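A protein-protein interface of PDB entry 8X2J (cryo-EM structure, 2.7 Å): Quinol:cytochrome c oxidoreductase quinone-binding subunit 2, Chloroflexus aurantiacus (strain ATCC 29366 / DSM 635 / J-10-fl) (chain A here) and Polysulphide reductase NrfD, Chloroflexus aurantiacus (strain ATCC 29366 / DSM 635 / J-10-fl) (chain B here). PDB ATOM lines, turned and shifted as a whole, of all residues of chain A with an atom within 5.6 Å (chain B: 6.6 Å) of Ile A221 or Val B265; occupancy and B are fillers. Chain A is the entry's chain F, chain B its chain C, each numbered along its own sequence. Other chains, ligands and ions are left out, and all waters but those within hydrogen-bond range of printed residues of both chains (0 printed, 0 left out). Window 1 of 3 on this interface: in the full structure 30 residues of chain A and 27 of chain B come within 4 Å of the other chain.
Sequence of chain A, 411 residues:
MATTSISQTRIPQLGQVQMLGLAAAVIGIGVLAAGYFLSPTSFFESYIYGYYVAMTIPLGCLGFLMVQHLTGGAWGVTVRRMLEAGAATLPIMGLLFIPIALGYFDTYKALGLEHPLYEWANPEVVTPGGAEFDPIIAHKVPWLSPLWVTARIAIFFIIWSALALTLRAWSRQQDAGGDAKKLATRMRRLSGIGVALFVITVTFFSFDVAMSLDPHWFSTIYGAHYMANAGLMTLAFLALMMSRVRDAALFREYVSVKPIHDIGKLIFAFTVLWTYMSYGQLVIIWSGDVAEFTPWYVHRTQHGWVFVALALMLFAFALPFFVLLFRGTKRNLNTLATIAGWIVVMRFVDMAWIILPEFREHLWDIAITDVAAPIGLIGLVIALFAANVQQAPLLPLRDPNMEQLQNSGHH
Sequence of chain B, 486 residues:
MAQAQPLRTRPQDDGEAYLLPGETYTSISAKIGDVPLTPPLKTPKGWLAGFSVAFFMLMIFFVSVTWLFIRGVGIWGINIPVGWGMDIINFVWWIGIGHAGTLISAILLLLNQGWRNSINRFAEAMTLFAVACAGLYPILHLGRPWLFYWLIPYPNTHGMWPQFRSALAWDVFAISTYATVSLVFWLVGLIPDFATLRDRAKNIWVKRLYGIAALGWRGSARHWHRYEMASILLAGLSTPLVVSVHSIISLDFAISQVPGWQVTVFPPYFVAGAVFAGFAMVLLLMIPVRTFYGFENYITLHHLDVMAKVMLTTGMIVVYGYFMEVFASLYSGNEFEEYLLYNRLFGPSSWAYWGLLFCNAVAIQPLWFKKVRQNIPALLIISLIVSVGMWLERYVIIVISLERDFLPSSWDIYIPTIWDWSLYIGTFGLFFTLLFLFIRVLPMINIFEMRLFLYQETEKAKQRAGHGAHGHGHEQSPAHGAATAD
Printed residues of chain B within 4 Å of Thr A220: Val B263 (3.7 Å), Thr B264 (3.3 Å), Val B265 (3.2 Å), Tyr B320 (3.98 Å) and Met B324 (3.3 Å).
Of chain B, only Thr B264 (3.3 Å), Val B265 (3.7 Å) and Pro B268 (3.8 Å) come within 4 Å of Ile A221.
Tyr A222 touches none of the printed residues of chain B.
Tyr A226 touches none of the printed residues of chain B.
Printed residues of chain B within 4 Å of Gln A281: Thr B264 (3.3 Å).
Printed residues of chain A within 4 Å of Thr B264: Ser A219, Thr A220, Ile A221, Gln A281 and Ile A284.
Of chain A, only Thr A220 and Ile A221 come within 4 Å of Val B265.
The nearest residue of chain B that does not touch Ile A221 is Pro B267 (4.8 Å).
The nearest residue of chain A that does not touch Val B265 is Ile A284 (5.2 Å).
Among the printed residues, pairs that only touch across the chains: Ser A219 with Thr B264 (3.3 Å), Gln A281 with Thr B264 (3.3 Å), Ile A221 with Thr B264 (3.3 Å), Thr A220 with Thr B264 (3.3 Å), Ala A224 with Tyr B320 (3.4 Å), Ile A284 with Thr B264 (3.7 Å), Thr A220 with Val B263 (3.7 Å), Ile A221 with Val B265 (3.7 Å), Ile A221 with Pro B268 (3.8 Å), Ile A284 with Pro B267 (3.8 Å) and Thr A220 with Tyr B320 (3.98 Å).
The backbone carbonyl oxygen (O) of Thr A220 lies close to the side-chain sulfur (SD) of Met B324.
OH of Tyr A276 sits close to N of Pro B268 (3.0 Å).
The backbone NH (N) of Val B265 is in hydrogen-bond range of the side-chain hydroxyl (OG1) of Thr A220, at 3.2 Å.
The side-chain hydroxyl of Tyr A276 sits close to the backbone carbonyl oxygen of Pro B267.
N of Tyr A222 lies within hydrogen-bond range of OG of Ser A219, 3.4 Å away.
Printed residues of chain A that touch a printed residue of chain B: Ser A219, Thr A220, Ile A221, Ala A224, Tyr A276, Gln A281 and Ile A284.
Hydrophobic or aromatic side chains of chain A that line the printed part of chain B: Ile A221, Ala A224, Tyr A276 and Ile A284.
Along chain B the printed residues that touch a printed residue of chain A span positions 263 to 324.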
ATOM      1  N   SER A 219      -4.469  -2.206  19.328  1.00  0.00           N
ATOM      2  CA  SER A 219      -4.991  -1.937  17.997  1.00  0.00           C
ATOM      3  C   SER A 219      -5.520  -3.240  17.423  1.00  0.00           C
ATOM      4  O   SER A 219      -4.841  -4.267  17.485  1.00  0.00           O
ATOM      5  CB  SER A 219      -3.912  -1.352  17.089  1.00  0.00           C
ATOM      6  OG  SER A 219      -4.306  -1.312  15.734  1.00  0.00           O
ATOM      7  N   THR A 220      -6.728  -3.192  16.875  1.00  0.00           N
ATOM      8  CA  THR A 220      -7.378  -4.376  16.338  1.00  0.00           C
ATOM      9  C   THR A 220      -7.107  -4.590  14.855  1.00  0.00           C
ATOM     10  O   THR A 220      -7.218  -5.725  14.381  1.00  0.00           O
ATOM     11  CB  THR A 220      -8.884  -4.291  16.592  1.00  0.00           C
ATOM     12  OG1 THR A 220      -9.349  -2.973  16.282  1.00  0.00           O
ATOM     13  CG2 THR A 220      -9.186  -4.582  18.041  1.00  0.00           C
ATOM     14  N   ILE A 221      -6.748  -3.536  14.112  1.00  0.00           N
ATOM     15  CA  ILE A 221      -6.294  -3.699  12.730  1.00  0.00           C
ATOM     16  C   ILE A 221      -4.859  -4.193  12.667  1.00  0.00           C
ATOM     17  O   ILE A 221      -4.402  -4.627  11.603  1.00  0.00           O
ATOM     18  CB  ILE A 221      -6.465  -2.380  11.950  1.00  0.00           C
ATOM     19  CG1 ILE A 221      -6.683  -2.643  10.458  1.00  0.00           C
ATOM     20  CG2 ILE A 221      -5.289  -1.454  12.164  1.00  0.00           C
ATOM     21  CD1 ILE A 221      -7.031  -1.413   9.660  1.00  0.00           C
ATOM     22  N   TYR A 222      -4.144  -4.144  13.784  1.00  0.00           N
ATOM     23  CA  TYR A 222      -2.838  -4.764  13.909  1.00  0.00           C
ATOM     24  C   TYR A 222      -2.984  -6.277  13.783  1.00  0.00           C
ATOM     25  O   TYR A 222      -4.020  -6.853  14.122  1.00  0.00           O
ATOM     26  CB  TYR A 222      -2.249  -4.403  15.265  1.00  0.00           C
ATOM     27  CG  TYR A 222      -0.747  -4.358  15.378  1.00  0.00           C
ATOM     28  CD1 TYR A 222      -0.012  -5.501  15.669  1.00  0.00           C
ATOM     29  CD2 TYR A 222      -0.067  -3.159  15.223  1.00  0.00           C
ATOM     30  CE1 TYR A 222       1.360  -5.448  15.792  1.00  0.00           C
ATOM     31  CE2 TYR A 222       1.298  -3.097  15.346  1.00  0.00           C
ATOM     32  CZ  TYR A 222       2.007  -4.241  15.627  1.00  0.00           C
ATOM     33  OH  TYR A 222       3.370  -4.163  15.739  1.00  0.00           O
ATOM     34  N   GLY A 223      -1.956  -6.919  13.273  1.00  0.00           N
ATOM     35  CA  GLY A 223      -2.074  -8.341  12.983  1.00  0.00           C
ATOM     36  C   GLY A 223      -2.578  -8.605  11.584  1.00  0.00           C
ATOM     37  O   GLY A 223      -1.970  -9.368  10.837  1.00  0.00           O
ATOM     38  N   ALA A 224      -3.693  -7.977  11.210  1.00  0.00           N
ATOM     39  CA  ALA A 224      -4.109  -7.977   9.815  1.00  0.00           C
ATOM     40  C   ALA A 224      -3.266  -7.015   8.989  1.00  0.00           C
ATOM     41  O   ALA A 224      -2.998  -7.276   7.808  1.00  0.00           O
ATOM     42  CB  ALA A 224      -5.591  -7.629   9.717  1.00  0.00           C
ATOM     43  N   HIS A 225      -2.823  -5.912   9.600  1.00  0.00           N
ATOM     44  CA  HIS A 225      -1.802  -5.072   8.983  1.00  0.00           C
ATOM     45  C   HIS A 225      -0.494  -5.835   8.835  1.00  0.00           C
ATOM     46  O   HIS A 225       0.206  -5.693   7.826  1.00  0.00           O
ATOM     47  CB  HIS A 225      -1.603  -3.802   9.811  1.00  0.00           C
ATOM     48  CG  HIS A 225      -0.375  -3.027   9.448  1.00  0.00           C
ATOM     49  ND1 HIS A 225      -0.320  -2.190   8.355  1.00  0.00           N
ATOM     50  CD2 HIS A 225       0.844  -2.961  10.033  1.00  0.00           C
ATOM     51  CE1 HIS A 225       0.879  -1.642   8.282  1.00  0.00           C
ATOM     52  NE2 HIS A 225       1.606  -2.095   9.287  1.00  0.00           N
ATOM     53  N   TYR A 226      -0.156  -6.665   9.825  1.00  0.00           N
ATOM     54  CA  TYR A 226       0.998  -7.548   9.701  1.00  0.00           C
ATOM     55  C   TYR A 226       0.788  -8.606   8.630  1.00  0.00           C
ATOM     56  O   TYR A 226       1.752  -9.026   7.986  1.00  0.00           O
ATOM     57  CB  TYR A 226       1.299  -8.219  11.037  1.00  0.00           C
ATOM     58  CG  TYR A 226       2.497  -9.137  10.990  1.00  0.00           C
ATOM     59  CD1 TYR A 226       3.737  -8.667  10.579  1.00  0.00           C
ATOM     60  CD2 TYR A 226       2.388 -10.474  11.350  1.00  0.00           C
ATOM     61  CE1 TYR A 226       4.836  -9.498  10.536  1.00  0.00           C
ATOM     62  CE2 TYR A 226       3.483 -11.315  11.308  1.00  0.00           C
ATOM     63  CZ  TYR A 226       4.704 -10.820  10.899  1.00  0.00           C
ATOM     64  OH  TYR A 226       5.798 -11.649  10.852  1.00  0.00           O
ATOM     65  N   TYR A 276      -3.145   1.020   2.835  1.00  0.00           N
ATOM     66  CA  TYR A 276      -4.510   1.140   3.331  1.00  0.00           C
ATOM     67  C   TYR A 276      -4.603   0.770   4.807  1.00  0.00           C
ATOM     68  O   TYR A 276      -5.202   1.504   5.601  1.00  0.00           O
ATOM     69  CB  TYR A 276      -5.411   0.249   2.484  1.00  0.00           C
ATOM     70  CG  TYR A 276      -6.723  -0.165   3.093  1.00  0.00           C
ATOM     71  CD1 TYR A 276      -7.698   0.774   3.411  1.00  0.00           C
ATOM     72  CD2 TYR A 276      -7.001  -1.503   3.318  1.00  0.00           C
ATOM     73  CE1 TYR A 276      -8.900   0.388   3.951  1.00  0.00           C
ATOM     74  CE2 TYR A 276      -8.197  -1.894   3.857  1.00  0.00           C
ATOM     75  CZ  TYR A 276      -9.137  -0.946   4.170  1.00  0.00           C
ATOM     76  OH  TYR A 276     -10.325  -1.343   4.698  1.00  0.00           O
ATOM     77  N   MET A 277      -4.024  -0.371   5.191  1.00  0.00           N
ATOM     78  CA  MET A 277      -4.080  -0.792   6.589  1.00  0.00           C
ATOM     79  C   MET A 277      -3.229   0.087   7.496  1.00  0.00           C
ATOM     80  O   MET A 277      -3.516   0.176   8.694  1.00  0.00           O
ATOM     81  CB  MET A 277      -3.643  -2.250   6.741  1.00  0.00           C
ATOM     82  CG  MET A 277      -4.398  -3.226   5.865  1.00  0.00           C
ATOM     83  SD  MET A 277      -6.126  -3.422   6.306  1.00  0.00           S
ATOM     84  CE  MET A 277      -6.010  -4.765   7.464  1.00  0.00           C
ATOM     85  N   GLY A 280      -5.459   3.634   7.557  1.00  0.00           N
ATOM     86  CA  GLY A 280      -6.698   3.533   8.313  1.00  0.00           C
ATOM     87  C   GLY A 280      -6.474   3.632   9.809  1.00  0.00           C
ATOM     88  O   GLY A 280      -7.156   4.396  10.496  1.00  0.00           O
ATOM     89  N   GLN A 281      -5.469   2.910  10.312  1.00  0.00           N
ATOM     90  CA  GLN A 281      -5.072   3.003  11.712  1.00  0.00           C
ATOM     91  C   GLN A 281      -4.585   4.400  12.065  1.00  0.00           C
ATOM     92  O   GLN A 281      -4.946   4.940  13.122  1.00  0.00           O
ATOM     93  CB  GLN A 281      -3.984   1.973  12.000  1.00  0.00           C
ATOM     94  CG  GLN A 281      -3.344   2.079  13.363  1.00  0.00           C
ATOM     95  CD  GLN A 281      -2.083   1.256  13.468  1.00  0.00           C
ATOM     96  OE1 GLN A 281      -1.749   0.493  12.564  1.00  0.00           O
ATOM     97  NE2 GLN A 281      -1.371   1.410  14.570  1.00  0.00           N
ATOM     98  N   ILE A 284      -7.571   6.856  12.097  1.00  0.00           N
ATOM     99  CA  ILE A 284      -8.472   6.582  13.213  1.00  0.00           C
ATOM    100  C   ILE A 284      -7.879   7.102  14.519  1.00  0.00           C
ATOM    101  O   ILE A 284      -8.548   7.810  15.281  1.00  0.00           O
ATOM    102  CB  ILE A 284      -8.795   5.078  13.277  1.00  0.00           C
ATOM    103  CG1 ILE A 284      -9.895   4.761  12.273  1.00  0.00           C
ATOM    104  CG2 ILE A 284      -9.251   4.657  14.660  1.00  0.00           C
ATOM    105  CD1 ILE A 284      -9.968   3.332  11.832  1.00  0.00           C
ATOM    106  N   SER B 250     -17.060   3.235   7.258  1.00  0.00           N
ATOM    107  CA  SER B 250     -16.564   2.815   8.566  1.00  0.00           C
ATOM    108  C   SER B 250     -16.033   3.999   9.361  1.00  0.00           C
ATOM    109  O   SER B 250     -16.163   4.053  10.590  1.00  0.00           O
ATOM    110  CB  SER B 250     -15.462   1.789   8.396  1.00  0.00           C
ATOM    111  OG  SER B 250     -14.241   2.447   8.123  1.00  0.00           O
ATOM    112  N   VAL B 263     -12.674   2.079  17.078  1.00  0.00           N
ATOM    113  CA  VAL B 263     -12.161   0.735  16.852  1.00  0.00           C
ATOM    114  C   VAL B 263     -11.485   0.762  15.493  1.00  0.00           C
ATOM    115  O   VAL B 263     -12.101   1.160  14.499  1.00  0.00           O
ATOM    116  CB  VAL B 263     -13.276  -0.329  16.891  1.00  0.00           C
ATOM    117  CG1 VAL B 263     -12.789  -1.641  16.318  1.00  0.00           C
ATOM    118  CG2 VAL B 263     -13.787  -0.534  18.303  1.00  0.00           C
ATOM    119  N   THR B 264     -10.221   0.363  15.447  1.00  0.00           N
ATOM    120  CA  THR B 264      -9.422   0.626  14.263  1.00  0.00           C
ATOM    121  C   THR B 264      -9.502  -0.464  13.200  1.00  0.00           C
ATOM    122  O   THR B 264      -8.996  -0.255  12.095  1.00  0.00           O
ATOM    123  CB  THR B 264      -7.969   0.867  14.663  1.00  0.00           C
ATOM    124  OG1 THR B 264      -7.223   1.282  13.518  1.00  0.00           O
ATOM    125  CG2 THR B 264      -7.379  -0.374  15.212  1.00  0.00           C
ATOM    126  N   VAL B 265     -10.150  -1.601  13.481  1.00  0.00           N
ATOM    127  CA  VAL B 265     -10.336  -2.633  12.465  1.00  0.00           C
ATOM    128  C   VAL B 265     -11.622  -2.397  11.671  1.00  0.00           C
ATOM    129  O   VAL B 265     -11.982  -3.217  10.811  1.00  0.00           O
ATOM    130  CB  VAL B 265     -10.312  -4.029  13.138  1.00  0.00           C
ATOM    131  CG1 VAL B 265     -11.568  -4.277  13.974  1.00  0.00           C
ATOM    132  CG2 VAL B 265      -9.925  -5.189  12.183  1.00  0.00           C
ATOM    133  N   PHE B 266     -12.329  -1.297  11.940  1.00  0.00           N
ATOM    134  CA  PHE B 266     -13.546  -0.977  11.195  1.00  0.00           C
ATOM    135  C   PHE B 266     -13.444  -0.839   9.678  1.00  0.00           C
ATOM    136  O   PHE B 266     -14.422  -1.223   9.025  1.00  0.00           O
ATOM    137  CB  PHE B 266     -14.261   0.270  11.742  1.00  0.00           C
ATOM    138  CG  PHE B 266     -15.015   0.039  13.020  1.00  0.00           C
ATOM    139  CD1 PHE B 266     -15.250  -1.246  13.480  1.00  0.00           C
ATOM    140  CD2 PHE B 266     -15.628   1.094  13.669  1.00  0.00           C
ATOM    141  CE1 PHE B 266     -15.990  -1.464  14.620  1.00  0.00           C
ATOM    142  CE2 PHE B 266     -16.376   0.881  14.806  1.00  0.00           C
ATOM    143  CZ  PHE B 266     -16.556  -0.399  15.282  1.00  0.00           C
ATOM    144  N   PRO B 267     -12.399  -0.291   9.046  1.00  0.00           N
ATOM    145  CA  PRO B 267     -12.420  -0.241   7.560  1.00  0.00           C
ATOM    146  C   PRO B 267     -12.397  -1.618   6.901  1.00  0.00           C
ATOM    147  O   PRO B 267     -13.293  -1.877   6.078  1.00  0.00           O
ATOM    148  CB  PRO B 267     -11.203   0.637   7.202  1.00  0.00           C
ATOM    149  CG  PRO B 267     -11.023   1.486   8.382  1.00  0.00           C
ATOM    150  CD  PRO B 267     -11.351   0.618   9.561  1.00  0.00           C
ATOM    151  N   PRO B 268     -11.489  -2.567   7.237  1.00  0.00           N
ATOM    152  CA  PRO B 268     -11.655  -3.897   6.620  1.00  0.00           C
ATOM    153  C   PRO B 268     -12.837  -4.675   7.178  1.00  0.00           C
ATOM    154  O   PRO B 268     -13.404  -5.508   6.460  1.00  0.00           O
ATOM    155  CB  PRO B 268     -10.324  -4.596   6.918  1.00  0.00           C
ATOM    156  CG  PRO B 268      -9.908  -4.036   8.173  1.00  0.00           C
ATOM    157  CD  PRO B 268     -10.277  -2.593   8.097  1.00  0.00           C
ATOM    158  N   TYR B 269     -13.246  -4.396   8.420  1.00  0.00           N
ATOM    159  CA  TYR B 269     -14.420  -5.037   9.001  1.00  0.00           C
ATOM    160  C   TYR B 269     -15.699  -4.623   8.280  1.00  0.00           C
ATOM    161  O   TYR B 269     -16.568  -5.461   8.011  1.00  0.00           O
ATOM    162  CB  TYR B 269     -14.468  -4.691  10.488  1.00  0.00           C
ATOM    163  CG  TYR B 269     -15.742  -5.000  11.224  1.00  0.00           C
ATOM    164  CD1 TYR B 269     -16.150  -6.310  11.440  1.00  0.00           C
ATOM    165  CD2 TYR B 269     -16.514  -3.978  11.750  1.00  0.00           C
ATOM    166  CE1 TYR B 269     -17.308  -6.586  12.140  1.00  0.00           C
ATOM    167  CE2 TYR B 269     -17.665  -4.240  12.449  1.00  0.00           C
ATOM    168  CZ  TYR B 269     -18.058  -5.543  12.641  1.00  0.00           C
ATOM    169  OH  TYR B 269     -19.213  -5.790  13.339  1.00  0.00           O
ATOM    170  N   PHE B 270     -15.811  -3.344   7.918  1.00  0.00           N
ATOM    171  CA  PHE B 270     -16.970  -2.851   7.186  1.00  0.00           C
ATOM    172  C   PHE B 270     -16.934  -3.282   5.732  1.00  0.00           C
ATOM    173  O   PHE B 270     -17.994  -3.520   5.144  1.00  0.00           O
ATOM    174  CB  PHE B 270     -17.040  -1.329   7.270  1.00  0.00           C
ATOM    175  CG  PHE B 270     -17.870  -0.814   8.412  1.00  0.00           C
ATOM    176  CD1 PHE B 270     -17.584  -1.181   9.718  1.00  0.00           C
ATOM    177  CD2 PHE B 270     -18.929   0.047   8.177  1.00  0.00           C
ATOM    178  CE1 PHE B 270     -18.344  -0.705  10.766  1.00  0.00           C
ATOM    179  CE2 PHE B 270     -19.690   0.527   9.220  1.00  0.00           C
ATOM    180  CZ  PHE B 270     -19.397   0.151  10.516  1.00  0.00           C
ATOM    181  N   TYR B 320     -14.202 -12.753  12.641  1.00  0.00           N
ATOM    182  CA  TYR B 320     -12.889 -12.333  13.124  1.00  0.00           C
ATOM    183  C   TYR B 320     -12.926 -10.904  13.660  1.00  0.00           C
ATOM    184  O   TYR B 320     -12.257 -10.589  14.648  1.00  0.00           O
ATOM    185  CB  TYR B 320     -11.865 -12.477  11.991  1.00  0.00           C
ATOM    186  CG  TYR B 320     -10.657 -11.567  12.067  1.00  0.00           C
ATOM    187  CD1 TYR B 320      -9.580 -11.879  12.886  1.00  0.00           C
ATOM    188  CD2 TYR B 320     -10.583 -10.406  11.298  1.00  0.00           C
ATOM    189  CE1 TYR B 320      -8.473 -11.058  12.951  1.00  0.00           C
ATOM    190  CE2 TYR B 320      -9.482  -9.575  11.366  1.00  0.00           C
ATOM    191  CZ  TYR B 320      -8.431  -9.908  12.190  1.00  0.00           C
ATOM    192  OH  TYR B 320      -7.333  -9.086  12.252  1.00  0.00           O
ATOM    193  N   GLY B 321     -13.706 -10.028  13.021  1.00  0.00           N
ATOM    194  CA  GLY B 321     -13.874  -8.673  13.535  1.00  0.00           C
ATOM    195  C   GLY B 321     -14.617  -8.620  14.861  1.00  0.00           C
ATOM    196  O   GLY B 321     -14.304  -7.790  15.725  1.00  0.00           O
ATOM    197  N   MET B 324     -12.109  -9.571  17.320  1.00  0.00           N
ATOM    198  CA  MET B 324     -11.205  -8.449  17.558  1.00  0.00           C
ATOM    199  C   MET B 324     -11.810  -7.435  18.519  1.00  0.00           C
ATOM    200  O   MET B 324     -11.114  -6.930  19.407  1.00  0.00           O
ATOM    201  CB  MET B 324     -10.840  -7.776  16.233  1.00  0.00           C
ATOM    202  CG  MET B 324      -9.808  -8.531  15.416  1.00  0.00           C
ATOM    203  SD  MET B 324      -8.255  -8.772  16.289  1.00  0.00           S
ATOM    204  CE  MET B 324      -8.280 -10.541  16.571  1.00  0.00           C
ATOM    205  N   GLU B 325     -13.104  -7.135  18.367  1.00  0.00           N
ATOM    206  CA  GLU B 325     -13.767  -6.212  19.291  1.00  0.00           C
ATOM    207  C   GLU B 325     -13.868  -6.794  20.701  1.00  0.00           C
ATOM    208  O   GLU B 325     -13.645  -6.080  21.690  1.00  0.00           O
ATOM    209  CB  GLU B 325     -15.154  -5.854  18.762  1.00  0.00           C
ATOM    210  CG  GLU B 325     -15.148  -4.847  17.630  1.00  0.00           C
ATOM    211  CD  GLU B 325     -16.541  -4.364  17.288  1.00  0.00           C
ATOM    212  OE1 GLU B 325     -17.374  -5.200  16.883  1.00  0.00           O
ATOM    213  OE2 GLU B 325     -16.805  -3.151  17.428  1.00  0.00           O
